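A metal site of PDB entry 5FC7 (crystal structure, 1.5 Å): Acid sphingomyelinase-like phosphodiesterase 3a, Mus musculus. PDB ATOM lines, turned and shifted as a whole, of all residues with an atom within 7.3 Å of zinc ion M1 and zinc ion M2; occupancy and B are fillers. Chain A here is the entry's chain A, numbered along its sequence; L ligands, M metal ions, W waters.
The backbone carbonyl oxygen (O) of His 237 is in hydrogen-bond range of the backbone NH (N) of Gly 277 (3.0 Å).
O of Asp 30 is in hydrogen-bond range of N of Thr 305, at 3.4 Å.
The backbone carbonyl oxygen (O) of Gly 94 sits at hydrogen-bond distance from the backbone NH (N) of Asp 30, at 2.9 Å.
The side-chain amide oxygen (OD1) of Asn 196 is in hydrogen-bond range of the backbone NH (N) of Asn 136, 3.0 Å away.
N of Asp 143 lies within hydrogen-bond range of O of Asn 136 (2.8 Å).
O of Pro 97 is in hydrogen-bond range of ND1 of His 32, at 2.8 Å.
The side-chain carboxylate (OD1) of Asp 95 sits at hydrogen-bond distance from the backbone NH (N) of His 137, 2.8 Å away.
The backbone carbonyl oxygen (O) of Asp 95 is in hydrogen-bond range of the backbone NH (N) of Leu 31 (3.3 Å).
Within 4 Å of zinc ion M1: Asp 95, Asn 136, His 237 and His 278.
Four residues have an atom within 4 Å of zinc ion M2: Asp 30, His 32, Asp 95 and His 280.
The nearest printed residue that does not touch zinc ion M2 is His 237 (4.1 Å).
A ring nitrogen (NE2) of His 237 is bound to zinc ion M1, at 2.0 Å.
An oxygen (O4) of the ligand is bound to zinc ion M1 (2.0 Å).
The side-chain amide oxygen (OD1) of Asn 136 is bound to zinc ion M1.
Zinc ion M1 is bound by ND1 of His 278 (2.2 Å).
Water W1 binds zinc ion M1 (2.3 Å).
Zinc ion M1 is bound by OD2 of Asp 95 (2.4 Å).
Zinc ion M1 has six donor atoms within binding distance.
Zinc ion M2 is bound by water W1 (2.0 Å), OD1 of Asp 30 (2.0 Å), NE2 of His 32 (2.1 Å), NE2 of His 280 (2.2 Å), O3 of the ligand (2.3 Å) and OD2 of Asp 95 (2.4 Å).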
ATOM      1  N   THR A  29      30.111  12.101  -2.413  1.00  0.00           N
ATOM      2  CA  THR A  29      30.116  10.688  -2.789  1.00  0.00           C
ATOM      3  C   THR A  29      29.084   9.892  -2.007  1.00  0.00           C
ATOM      4  O   THR A  29      28.674  10.252  -0.902  1.00  0.00           O
ATOM      5  CB  THR A  29      31.527  10.079  -2.663  1.00  0.00           C
ATOM      6  OG1 THR A  29      31.606   8.815  -3.357  1.00  0.00           O
ATOM      7  CG2 THR A  29      31.938   9.908  -1.259  1.00  0.00           C
ATOM      8  N   ASP A  30      28.665   8.791  -2.602  1.00  0.00           N
ATOM      9  CA  ASP A  30      27.868   7.769  -1.934  1.00  0.00           C
ATOM     10  C   ASP A  30      26.615   8.385  -1.296  1.00  0.00           C
ATOM     11  O   ASP A  30      26.396   8.282  -0.087  1.00  0.00           O
ATOM     12  CB  ASP A  30      28.739   7.008  -0.918  1.00  0.00           C
ATOM     13  CG  ASP A  30      29.773   6.142  -1.603  1.00  0.00           C
ATOM     14  OD1 ASP A  30      29.427   4.975  -1.891  1.00  0.00           O
ATOM     15  OD2 ASP A  30      30.922   6.623  -1.863  1.00  0.00           O
ATOM     16  N   LEU A  31      25.814   9.034  -2.161  1.00  0.00           N
ATOM     17  CA  LEU A  31      24.581   9.678  -1.739  1.00  0.00           C
ATOM     18  C   LEU A  31      23.529   8.660  -1.307  1.00  0.00           C
ATOM     19  O   LEU A  31      22.812   8.868  -0.324  1.00  0.00           O
ATOM     20  CB  LEU A  31      24.053  10.570  -2.868  1.00  0.00           C
ATOM     21  CG  LEU A  31      25.008  11.703  -3.306  1.00  0.00           C
ATOM     22  CD1 LEU A  31      24.421  12.509  -4.491  1.00  0.00           C
ATOM     23  CD2 LEU A  31      25.344  12.658  -2.165  1.00  0.00           C
ATOM     24  N   HIS A  32      23.428   7.554  -2.049  1.00  0.00           N
ATOM     25  CA  HIS A  32      22.521   6.453  -1.739  1.00  0.00           C
ATOM     26  C   HIS A  32      21.149   6.946  -1.287  1.00  0.00           C
ATOM     27  O   HIS A  32      20.699   6.706  -0.166  1.00  0.00           O
ATOM     28  CB  HIS A  32      23.119   5.514  -0.706  1.00  0.00           C
ATOM     29  CG  HIS A  32      24.319   4.753  -1.170  1.00  0.00           C
ATOM     30  ND1 HIS A  32      24.248   3.668  -2.016  1.00  0.00           N
ATOM     31  CD2 HIS A  32      25.622   4.871  -0.820  1.00  0.00           C
ATOM     32  CE1 HIS A  32      25.461   3.161  -2.180  1.00  0.00           C
ATOM     33  NE2 HIS A  32      26.308   3.871  -1.450  1.00  0.00           N
ATOM     34  N   ASP A  67      19.426   4.093   4.304  1.00  0.00           N
ATOM     35  CA  ASP A  67      20.056   5.010   3.371  1.00  0.00           C
ATOM     36  C   ASP A  67      19.404   6.387   3.464  1.00  0.00           C
ATOM     37  O   ASP A  67      18.515   6.641   4.275  1.00  0.00           O
ATOM     38  CB  ASP A  67      20.051   4.407   1.994  1.00  0.00           C
ATOM     39  CG  ASP A  67      21.279   3.577   1.753  1.00  0.00           C
ATOM     40  OD1 ASP A  67      22.378   4.003   2.162  1.00  0.00           O
ATOM     41  OD2 ASP A  67      21.154   2.464   1.209  1.00  0.00           O
ATOM     42  N   THR A  93      31.656  11.006  -6.800  1.00  0.00           N
ATOM     43  CA  THR A  93      32.204   9.684  -7.104  1.00  0.00           C
ATOM     44  C   THR A  93      31.258   8.512  -6.903  1.00  0.00           C
ATOM     45  O   THR A  93      31.688   7.436  -6.484  1.00  0.00           O
ATOM     46  CB  THR A  93      33.550   9.443  -6.402  1.00  0.00           C
ATOM     47  OG1 THR A  93      33.473   9.825  -5.047  1.00  0.00           O
ATOM     48  CG2 THR A  93      34.622  10.310  -7.030  1.00  0.00           C
ATOM     49  N   GLY A  94      29.969   8.677  -7.230  1.00  0.00           N
ATOM     50  CA  GLY A  94      29.087   7.555  -7.498  1.00  0.00           C
ATOM     51  C   GLY A  94      28.274   7.040  -6.320  1.00  0.00           C
ATOM     52  O   GLY A  94      28.313   7.549  -5.185  1.00  0.00           O
ATOM     53  N   ASP A  95      27.488   6.005  -6.628  1.00  0.00           N
ATOM     54  CA  ASP A  95      26.652   5.239  -5.688  1.00  0.00           C
ATOM     55  C   ASP A  95      25.392   5.974  -5.275  1.00  0.00           C
ATOM     56  O   ASP A  95      25.223   6.371  -4.104  1.00  0.00           O
ATOM     57  CB  ASP A  95      27.438   4.743  -4.492  1.00  0.00           C
ATOM     58  CG  ASP A  95      27.844   3.266  -4.615  1.00  0.00           C
ATOM     59  OD1 ASP A  95      27.738   2.699  -5.701  1.00  0.00           O
ATOM     60  OD2 ASP A  95      28.321   2.665  -3.616  1.00  0.00           O
ATOM     61  N   SER A  96      24.474   6.093  -6.211  1.00  0.00           N
ATOM     62  CA  SER A  96      23.260   6.861  -5.970  1.00  0.00           C
ATOM     63  C   SER A  96      22.044   6.045  -5.525  1.00  0.00           C
ATOM     64  O   SER A  96      21.311   6.521  -4.664  1.00  0.00           O
ATOM     65  CB  SER A  96      22.945   7.749  -7.175  1.00  0.00           C
ATOM     66  OG  SER A  96      23.934   8.769  -7.300  1.00  0.00           O
ATOM     67  N   PRO A  97      21.777   4.863  -6.062  1.00  0.00           N
ATOM     68  CA  PRO A  97      20.618   4.085  -5.575  1.00  0.00           C
ATOM     69  C   PRO A  97      20.888   3.475  -4.206  1.00  0.00           C
ATOM     70  O   PRO A  97      22.034   3.357  -3.766  1.00  0.00           O
ATOM     71  CB  PRO A  97      20.479   2.983  -6.638  1.00  0.00           C
ATOM     72  CG  PRO A  97      21.234   3.472  -7.822  1.00  0.00           C
ATOM     73  CD  PRO A  97      22.374   4.245  -7.252  1.00  0.00           C
ATOM     74  N   HIS A  99      20.723   0.650  -0.882  1.00  0.00           N
ATOM     75  CA  HIS A  99      21.059  -0.749  -0.604  1.00  0.00           C
ATOM     76  C   HIS A  99      19.753  -1.465  -0.331  1.00  0.00           C
ATOM     77  O   HIS A  99      19.309  -1.630   0.811  1.00  0.00           O
ATOM     78  CB  HIS A  99      21.978  -0.860   0.610  1.00  0.00           C
ATOM     79  CG  HIS A  99      23.299  -0.160   0.448  1.00  0.00           C
ATOM     80  ND1 HIS A  99      23.438   1.195   0.654  1.00  0.00           N
ATOM     81  CD2 HIS A  99      24.512  -0.602   0.038  1.00  0.00           C
ATOM     82  CE1 HIS A  99      24.690   1.539   0.440  1.00  0.00           C
ATOM     83  NE2 HIS A  99      25.358   0.477   0.062  1.00  0.00           N
ATOM     84  N   GLY A 135      29.404   4.473  -9.629  1.00  0.00           N
ATOM     85  CA  GLY A 135      29.636   3.568  -8.514  1.00  0.00           C
ATOM     86  C   GLY A 135      29.074   2.176  -8.788  1.00  0.00           C
ATOM     87  O   GLY A 135      28.366   1.956  -9.778  1.00  0.00           O
ATOM     88  N   ASN A 136      29.401   1.217  -7.905  1.00  0.00           N
ATOM     89  CA  ASN A 136      28.991  -0.159  -8.162  1.00  0.00           C
ATOM     90  C   ASN A 136      27.479  -0.326  -8.043  1.00  0.00           C
ATOM     91  O   ASN A 136      26.929  -1.238  -8.670  1.00  0.00           O
ATOM     92  CB  ASN A 136      29.726  -1.162  -7.259  1.00  0.00           C
ATOM     93  CG  ASN A 136      29.650  -0.805  -5.800  1.00  0.00           C
ATOM     94  OD1 ASN A 136      30.135   0.247  -5.391  1.00  0.00           O
ATOM     95  ND2 ASN A 136      29.030  -1.666  -5.002  1.00  0.00           N
ATOM     96  N   HIS A 137      26.782   0.545  -7.286  1.00  0.00           N
ATOM     97  CA  HIS A 137      25.338   0.507  -7.229  1.00  0.00           C
ATOM     98  C   HIS A 137      24.682   1.256  -8.388  1.00  0.00           C
ATOM     99  O   HIS A 137      23.446   1.190  -8.535  1.00  0.00           O
ATOM    100  CB  HIS A 137      24.809   1.048  -5.902  1.00  0.00           C
ATOM    101  CG  HIS A 137      25.089   0.161  -4.754  1.00  0.00           C
ATOM    102  ND1 HIS A 137      24.197  -0.800  -4.325  1.00  0.00           N
ATOM    103  CD2 HIS A 137      26.200   0.028  -3.990  1.00  0.00           C
ATOM    104  CE1 HIS A 137      24.732  -1.457  -3.319  1.00  0.00           C
ATOM    105  NE2 HIS A 137      25.938  -0.970  -3.084  1.00  0.00           N
ATOM    106  N   ASP A 143      26.776  -4.019  -9.174  1.00  0.00           N
ATOM    107  CA  ASP A 143      28.125  -4.544  -9.302  1.00  0.00           C
ATOM    108  C   ASP A 143      28.437  -5.108 -10.683  1.00  0.00           C
ATOM    109  O   ASP A 143      29.603  -5.332 -10.977  1.00  0.00           O
ATOM    110  CB  ASP A 143      28.453  -5.625  -8.253  1.00  0.00           C
ATOM    111  CG  ASP A 143      28.127  -5.192  -6.834  1.00  0.00           C
ATOM    112  OD1 ASP A 143      28.189  -3.985  -6.553  1.00  0.00           O
ATOM    113  OD2 ASP A 143      27.815  -6.079  -5.994  1.00  0.00           O
ATOM    114  N   ASN A 196      34.783  -0.017 -10.977  1.00  0.00           N
ATOM    115  CA  ASN A 196      33.857  -1.117 -10.728  1.00  0.00           C
ATOM    116  C   ASN A 196      34.128  -2.275 -11.685  1.00  0.00           C
ATOM    117  O   ASN A 196      33.712  -3.401 -11.407  1.00  0.00           O
ATOM    118  CB  ASN A 196      32.429  -0.615 -10.888  1.00  0.00           C
ATOM    119  CG  ASN A 196      32.180   0.644 -10.116  1.00  0.00           C
ATOM    120  OD1 ASN A 196      32.155   0.644  -8.884  1.00  0.00           O
ATOM    121  ND2 ASN A 196      32.036   1.745 -10.828  1.00  0.00           N
ATOM    122  N   TYR A 199      36.160  -4.567  -9.437  1.00  0.00           N
ATOM    123  CA  TYR A 199      35.629  -4.875  -8.133  1.00  0.00           C
ATOM    124  C   TYR A 199      35.233  -6.342  -8.090  1.00  0.00           C
ATOM    125  O   TYR A 199      34.636  -6.885  -9.046  1.00  0.00           O
ATOM    126  CB  TYR A 199      34.421  -3.959  -7.961  1.00  0.00           C
ATOM    127  CG  TYR A 199      33.722  -4.007  -6.631  1.00  0.00           C
ATOM    128  CD1 TYR A 199      34.417  -4.014  -5.440  1.00  0.00           C
ATOM    129  CD2 TYR A 199      32.332  -4.046  -6.576  1.00  0.00           C
ATOM    130  CE1 TYR A 199      33.738  -4.059  -4.200  1.00  0.00           C
ATOM    131  CE2 TYR A 199      31.627  -4.047  -5.389  1.00  0.00           C
ATOM    132  CZ  TYR A 199      32.343  -4.076  -4.186  1.00  0.00           C
ATOM    133  OH  TYR A 199      31.684  -4.144  -2.956  1.00  0.00           O
ATOM    134  N   HIS A 237      35.120   5.525  -8.086  1.00  0.00           N
ATOM    135  CA  HIS A 237      34.326   5.059  -6.953  1.00  0.00           C
ATOM    136  C   HIS A 237      35.161   4.168  -6.028  1.00  0.00           C
ATOM    137  O   HIS A 237      35.554   4.599  -4.947  1.00  0.00           O
ATOM    138  CB  HIS A 237      33.046   4.360  -7.425  1.00  0.00           C
ATOM    139  CG  HIS A 237      32.186   3.922  -6.277  1.00  0.00           C
ATOM    140  ND1 HIS A 237      31.563   4.816  -5.442  1.00  0.00           N
ATOM    141  CD2 HIS A 237      31.858   2.684  -5.809  1.00  0.00           C
ATOM    142  CE1 HIS A 237      30.882   4.165  -4.514  1.00  0.00           C
ATOM    143  NE2 HIS A 237      31.046   2.864  -4.713  1.00  0.00           N
ATOM    144  N   VAL A 238      35.479   2.949  -6.468  1.00  0.00           N
ATOM    145  CA  VAL A 238      36.225   2.025  -5.628  1.00  0.00           C
ATOM    146  C   VAL A 238      37.699   2.429  -5.645  1.00  0.00           C
ATOM    147  O   VAL A 238      38.286   2.591  -6.735  1.00  0.00           O
ATOM    148  CB  VAL A 238      36.052   0.581  -6.122  1.00  0.00           C
ATOM    149  CG1 VAL A 238      36.688  -0.369  -5.099  1.00  0.00           C
ATOM    150  CG2 VAL A 238      34.599   0.256  -6.384  1.00  0.00           C
ATOM    151  N   GLY A 277      35.688   7.101  -3.370  1.00  0.00           N
ATOM    152  CA  GLY A 277      34.604   6.902  -2.408  1.00  0.00           C
ATOM    153  C   GLY A 277      34.496   5.438  -2.005  1.00  0.00           C
ATOM    154  O   GLY A 277      35.521   4.802  -1.689  1.00  0.00           O
ATOM    155  N   HIS A 278      33.268   4.910  -2.027  1.00  0.00           N
ATOM    156  CA  HIS A 278      32.923   3.498  -1.830  1.00  0.00           C
ATOM    157  C   HIS A 278      33.036   2.976  -0.397  1.00  0.00           C
ATOM    158  O   HIS A 278      32.166   2.220   0.038  1.00  0.00           O
ATOM    159  CB  HIS A 278      33.734   2.621  -2.766  1.00  0.00           C
ATOM    160  CG  HIS A 278      33.447   1.164  -2.647  1.00  0.00           C
ATOM    161  ND1 HIS A 278      32.254   0.605  -3.038  1.00  0.00           N
ATOM    162  CD2 HIS A 278      34.209   0.149  -2.165  1.00  0.00           C
ATOM    163  CE1 HIS A 278      32.276  -0.700  -2.775  1.00  0.00           C
ATOM    164  NE2 HIS A 278      33.470  -1.002  -2.277  1.00  0.00           N
ATOM    165  N   THR A 279      34.097   3.335   0.332  1.00  0.00           N
ATOM    166  CA  THR A 279      34.274   2.773   1.669  1.00  0.00           C
ATOM    167  C   THR A 279      33.378   3.413   2.709  1.00  0.00           C
ATOM    168  O   THR A 279      33.191   2.819   3.792  1.00  0.00           O
ATOM    169  CB  THR A 279      35.719   2.887   2.126  1.00  0.00           C
ATOM    170  OG1 THR A 279      36.006   4.241   2.419  1.00  0.00           O
ATOM    171  CG2 THR A 279      36.697   2.324   1.059  1.00  0.00           C
ATOM    172  N   HIS A 280      32.809   4.587   2.407  1.00  0.00           N
ATOM    173  CA  HIS A 280      31.970   5.351   3.314  1.00  0.00           C
ATOM    174  C   HIS A 280      32.743   5.825   4.559  1.00  0.00           C
ATOM    175  O   HIS A 280      32.134   6.139   5.578  1.00  0.00           O
ATOM    176  CB  HIS A 280      30.703   4.611   3.738  1.00  0.00           C
ATOM    177  CG  HIS A 280      29.749   4.242   2.628  1.00  0.00           C
ATOM    178  ND1 HIS A 280      28.453   3.856   2.902  1.00  0.00           N
ATOM    179  CD2 HIS A 280      29.880   4.194   1.281  1.00  0.00           C
ATOM    180  CE1 HIS A 280      27.827   3.596   1.756  1.00  0.00           C
ATOM    181  NE2 HIS A 280      28.677   3.797   0.763  1.00  0.00           N
ATOM    182  N   ALA A 303      30.837   8.975   3.085  1.00  0.00           N
ATOM    183  CA  ALA A 303      29.566   9.039   2.409  1.00  0.00           C
ATOM    184  C   ALA A 303      28.635  10.093   3.017  1.00  0.00           C
ATOM    185  O   ALA A 303      28.773  10.511   4.176  1.00  0.00           O
ATOM    186  CB  ALA A 303      28.864   7.693   2.535  1.00  0.00           C
ATOM    187  N   THR A 305      25.314   9.043   2.992  1.00  0.00           N
ATOM    188  CA  THR A 305      24.497   8.079   3.722  1.00  0.00           C
ATOM    189  C   THR A 305      25.204   7.637   5.002  1.00  0.00           C
ATOM    190  O   THR A 305      26.447   7.446   5.009  1.00  0.00           O
ATOM    191  CB  THR A 305      24.165   6.846   2.884  1.00  0.00           C
ATOM    192  OG1 THR A 305      23.268   5.997   3.625  1.00  0.00           O
ATOM    193  CG2 THR A 305      25.433   6.045   2.511  1.00  0.00           C
ATOM    194  N   VAL A 307      24.267   4.706   6.419  1.00  0.00           N
ATOM    195  CA  VAL A 307      23.751   3.339   6.542  1.00  0.00           C
ATOM    196  C   VAL A 307      24.793   2.374   7.097  1.00  0.00           C
ATOM    197  O   VAL A 307      25.985   2.443   6.767  1.00  0.00           O
ATOM    198  CB  VAL A 307      23.213   2.865   5.175  1.00  0.00           C
ATOM    199  CG1 VAL A 307      24.364   2.582   4.180  1.00  0.00           C
ATOM    200  CG2 VAL A 307      22.298   1.666   5.326  1.00  0.00           C
HETATM  201  S1  LIG L   1      28.775  -0.016  -1.199  1.00  0.00           S
HETATM  202  O1  LIG L   1      29.809  -0.264  -0.154  1.00  0.00           O
HETATM  203  O2  LIG L   1      27.854  -1.207  -1.071  1.00  0.00           O
HETATM  204  O3  LIG L   1      27.920   1.153  -0.918  1.00  0.00           O
HETATM  205  O4  LIG L   1      29.255  -0.062  -2.592  1.00  0.00           O
HETATM  206 ZN    ZN M   1      30.289   1.349  -3.653  1.00  0.00          ZN
HETATM  207 ZN    ZN M   2      28.348   3.353  -1.341  1.00  0.00          ZN
HETATM  208  O   HOH W   1      29.927   2.226  -1.562  1.00  0.00           O
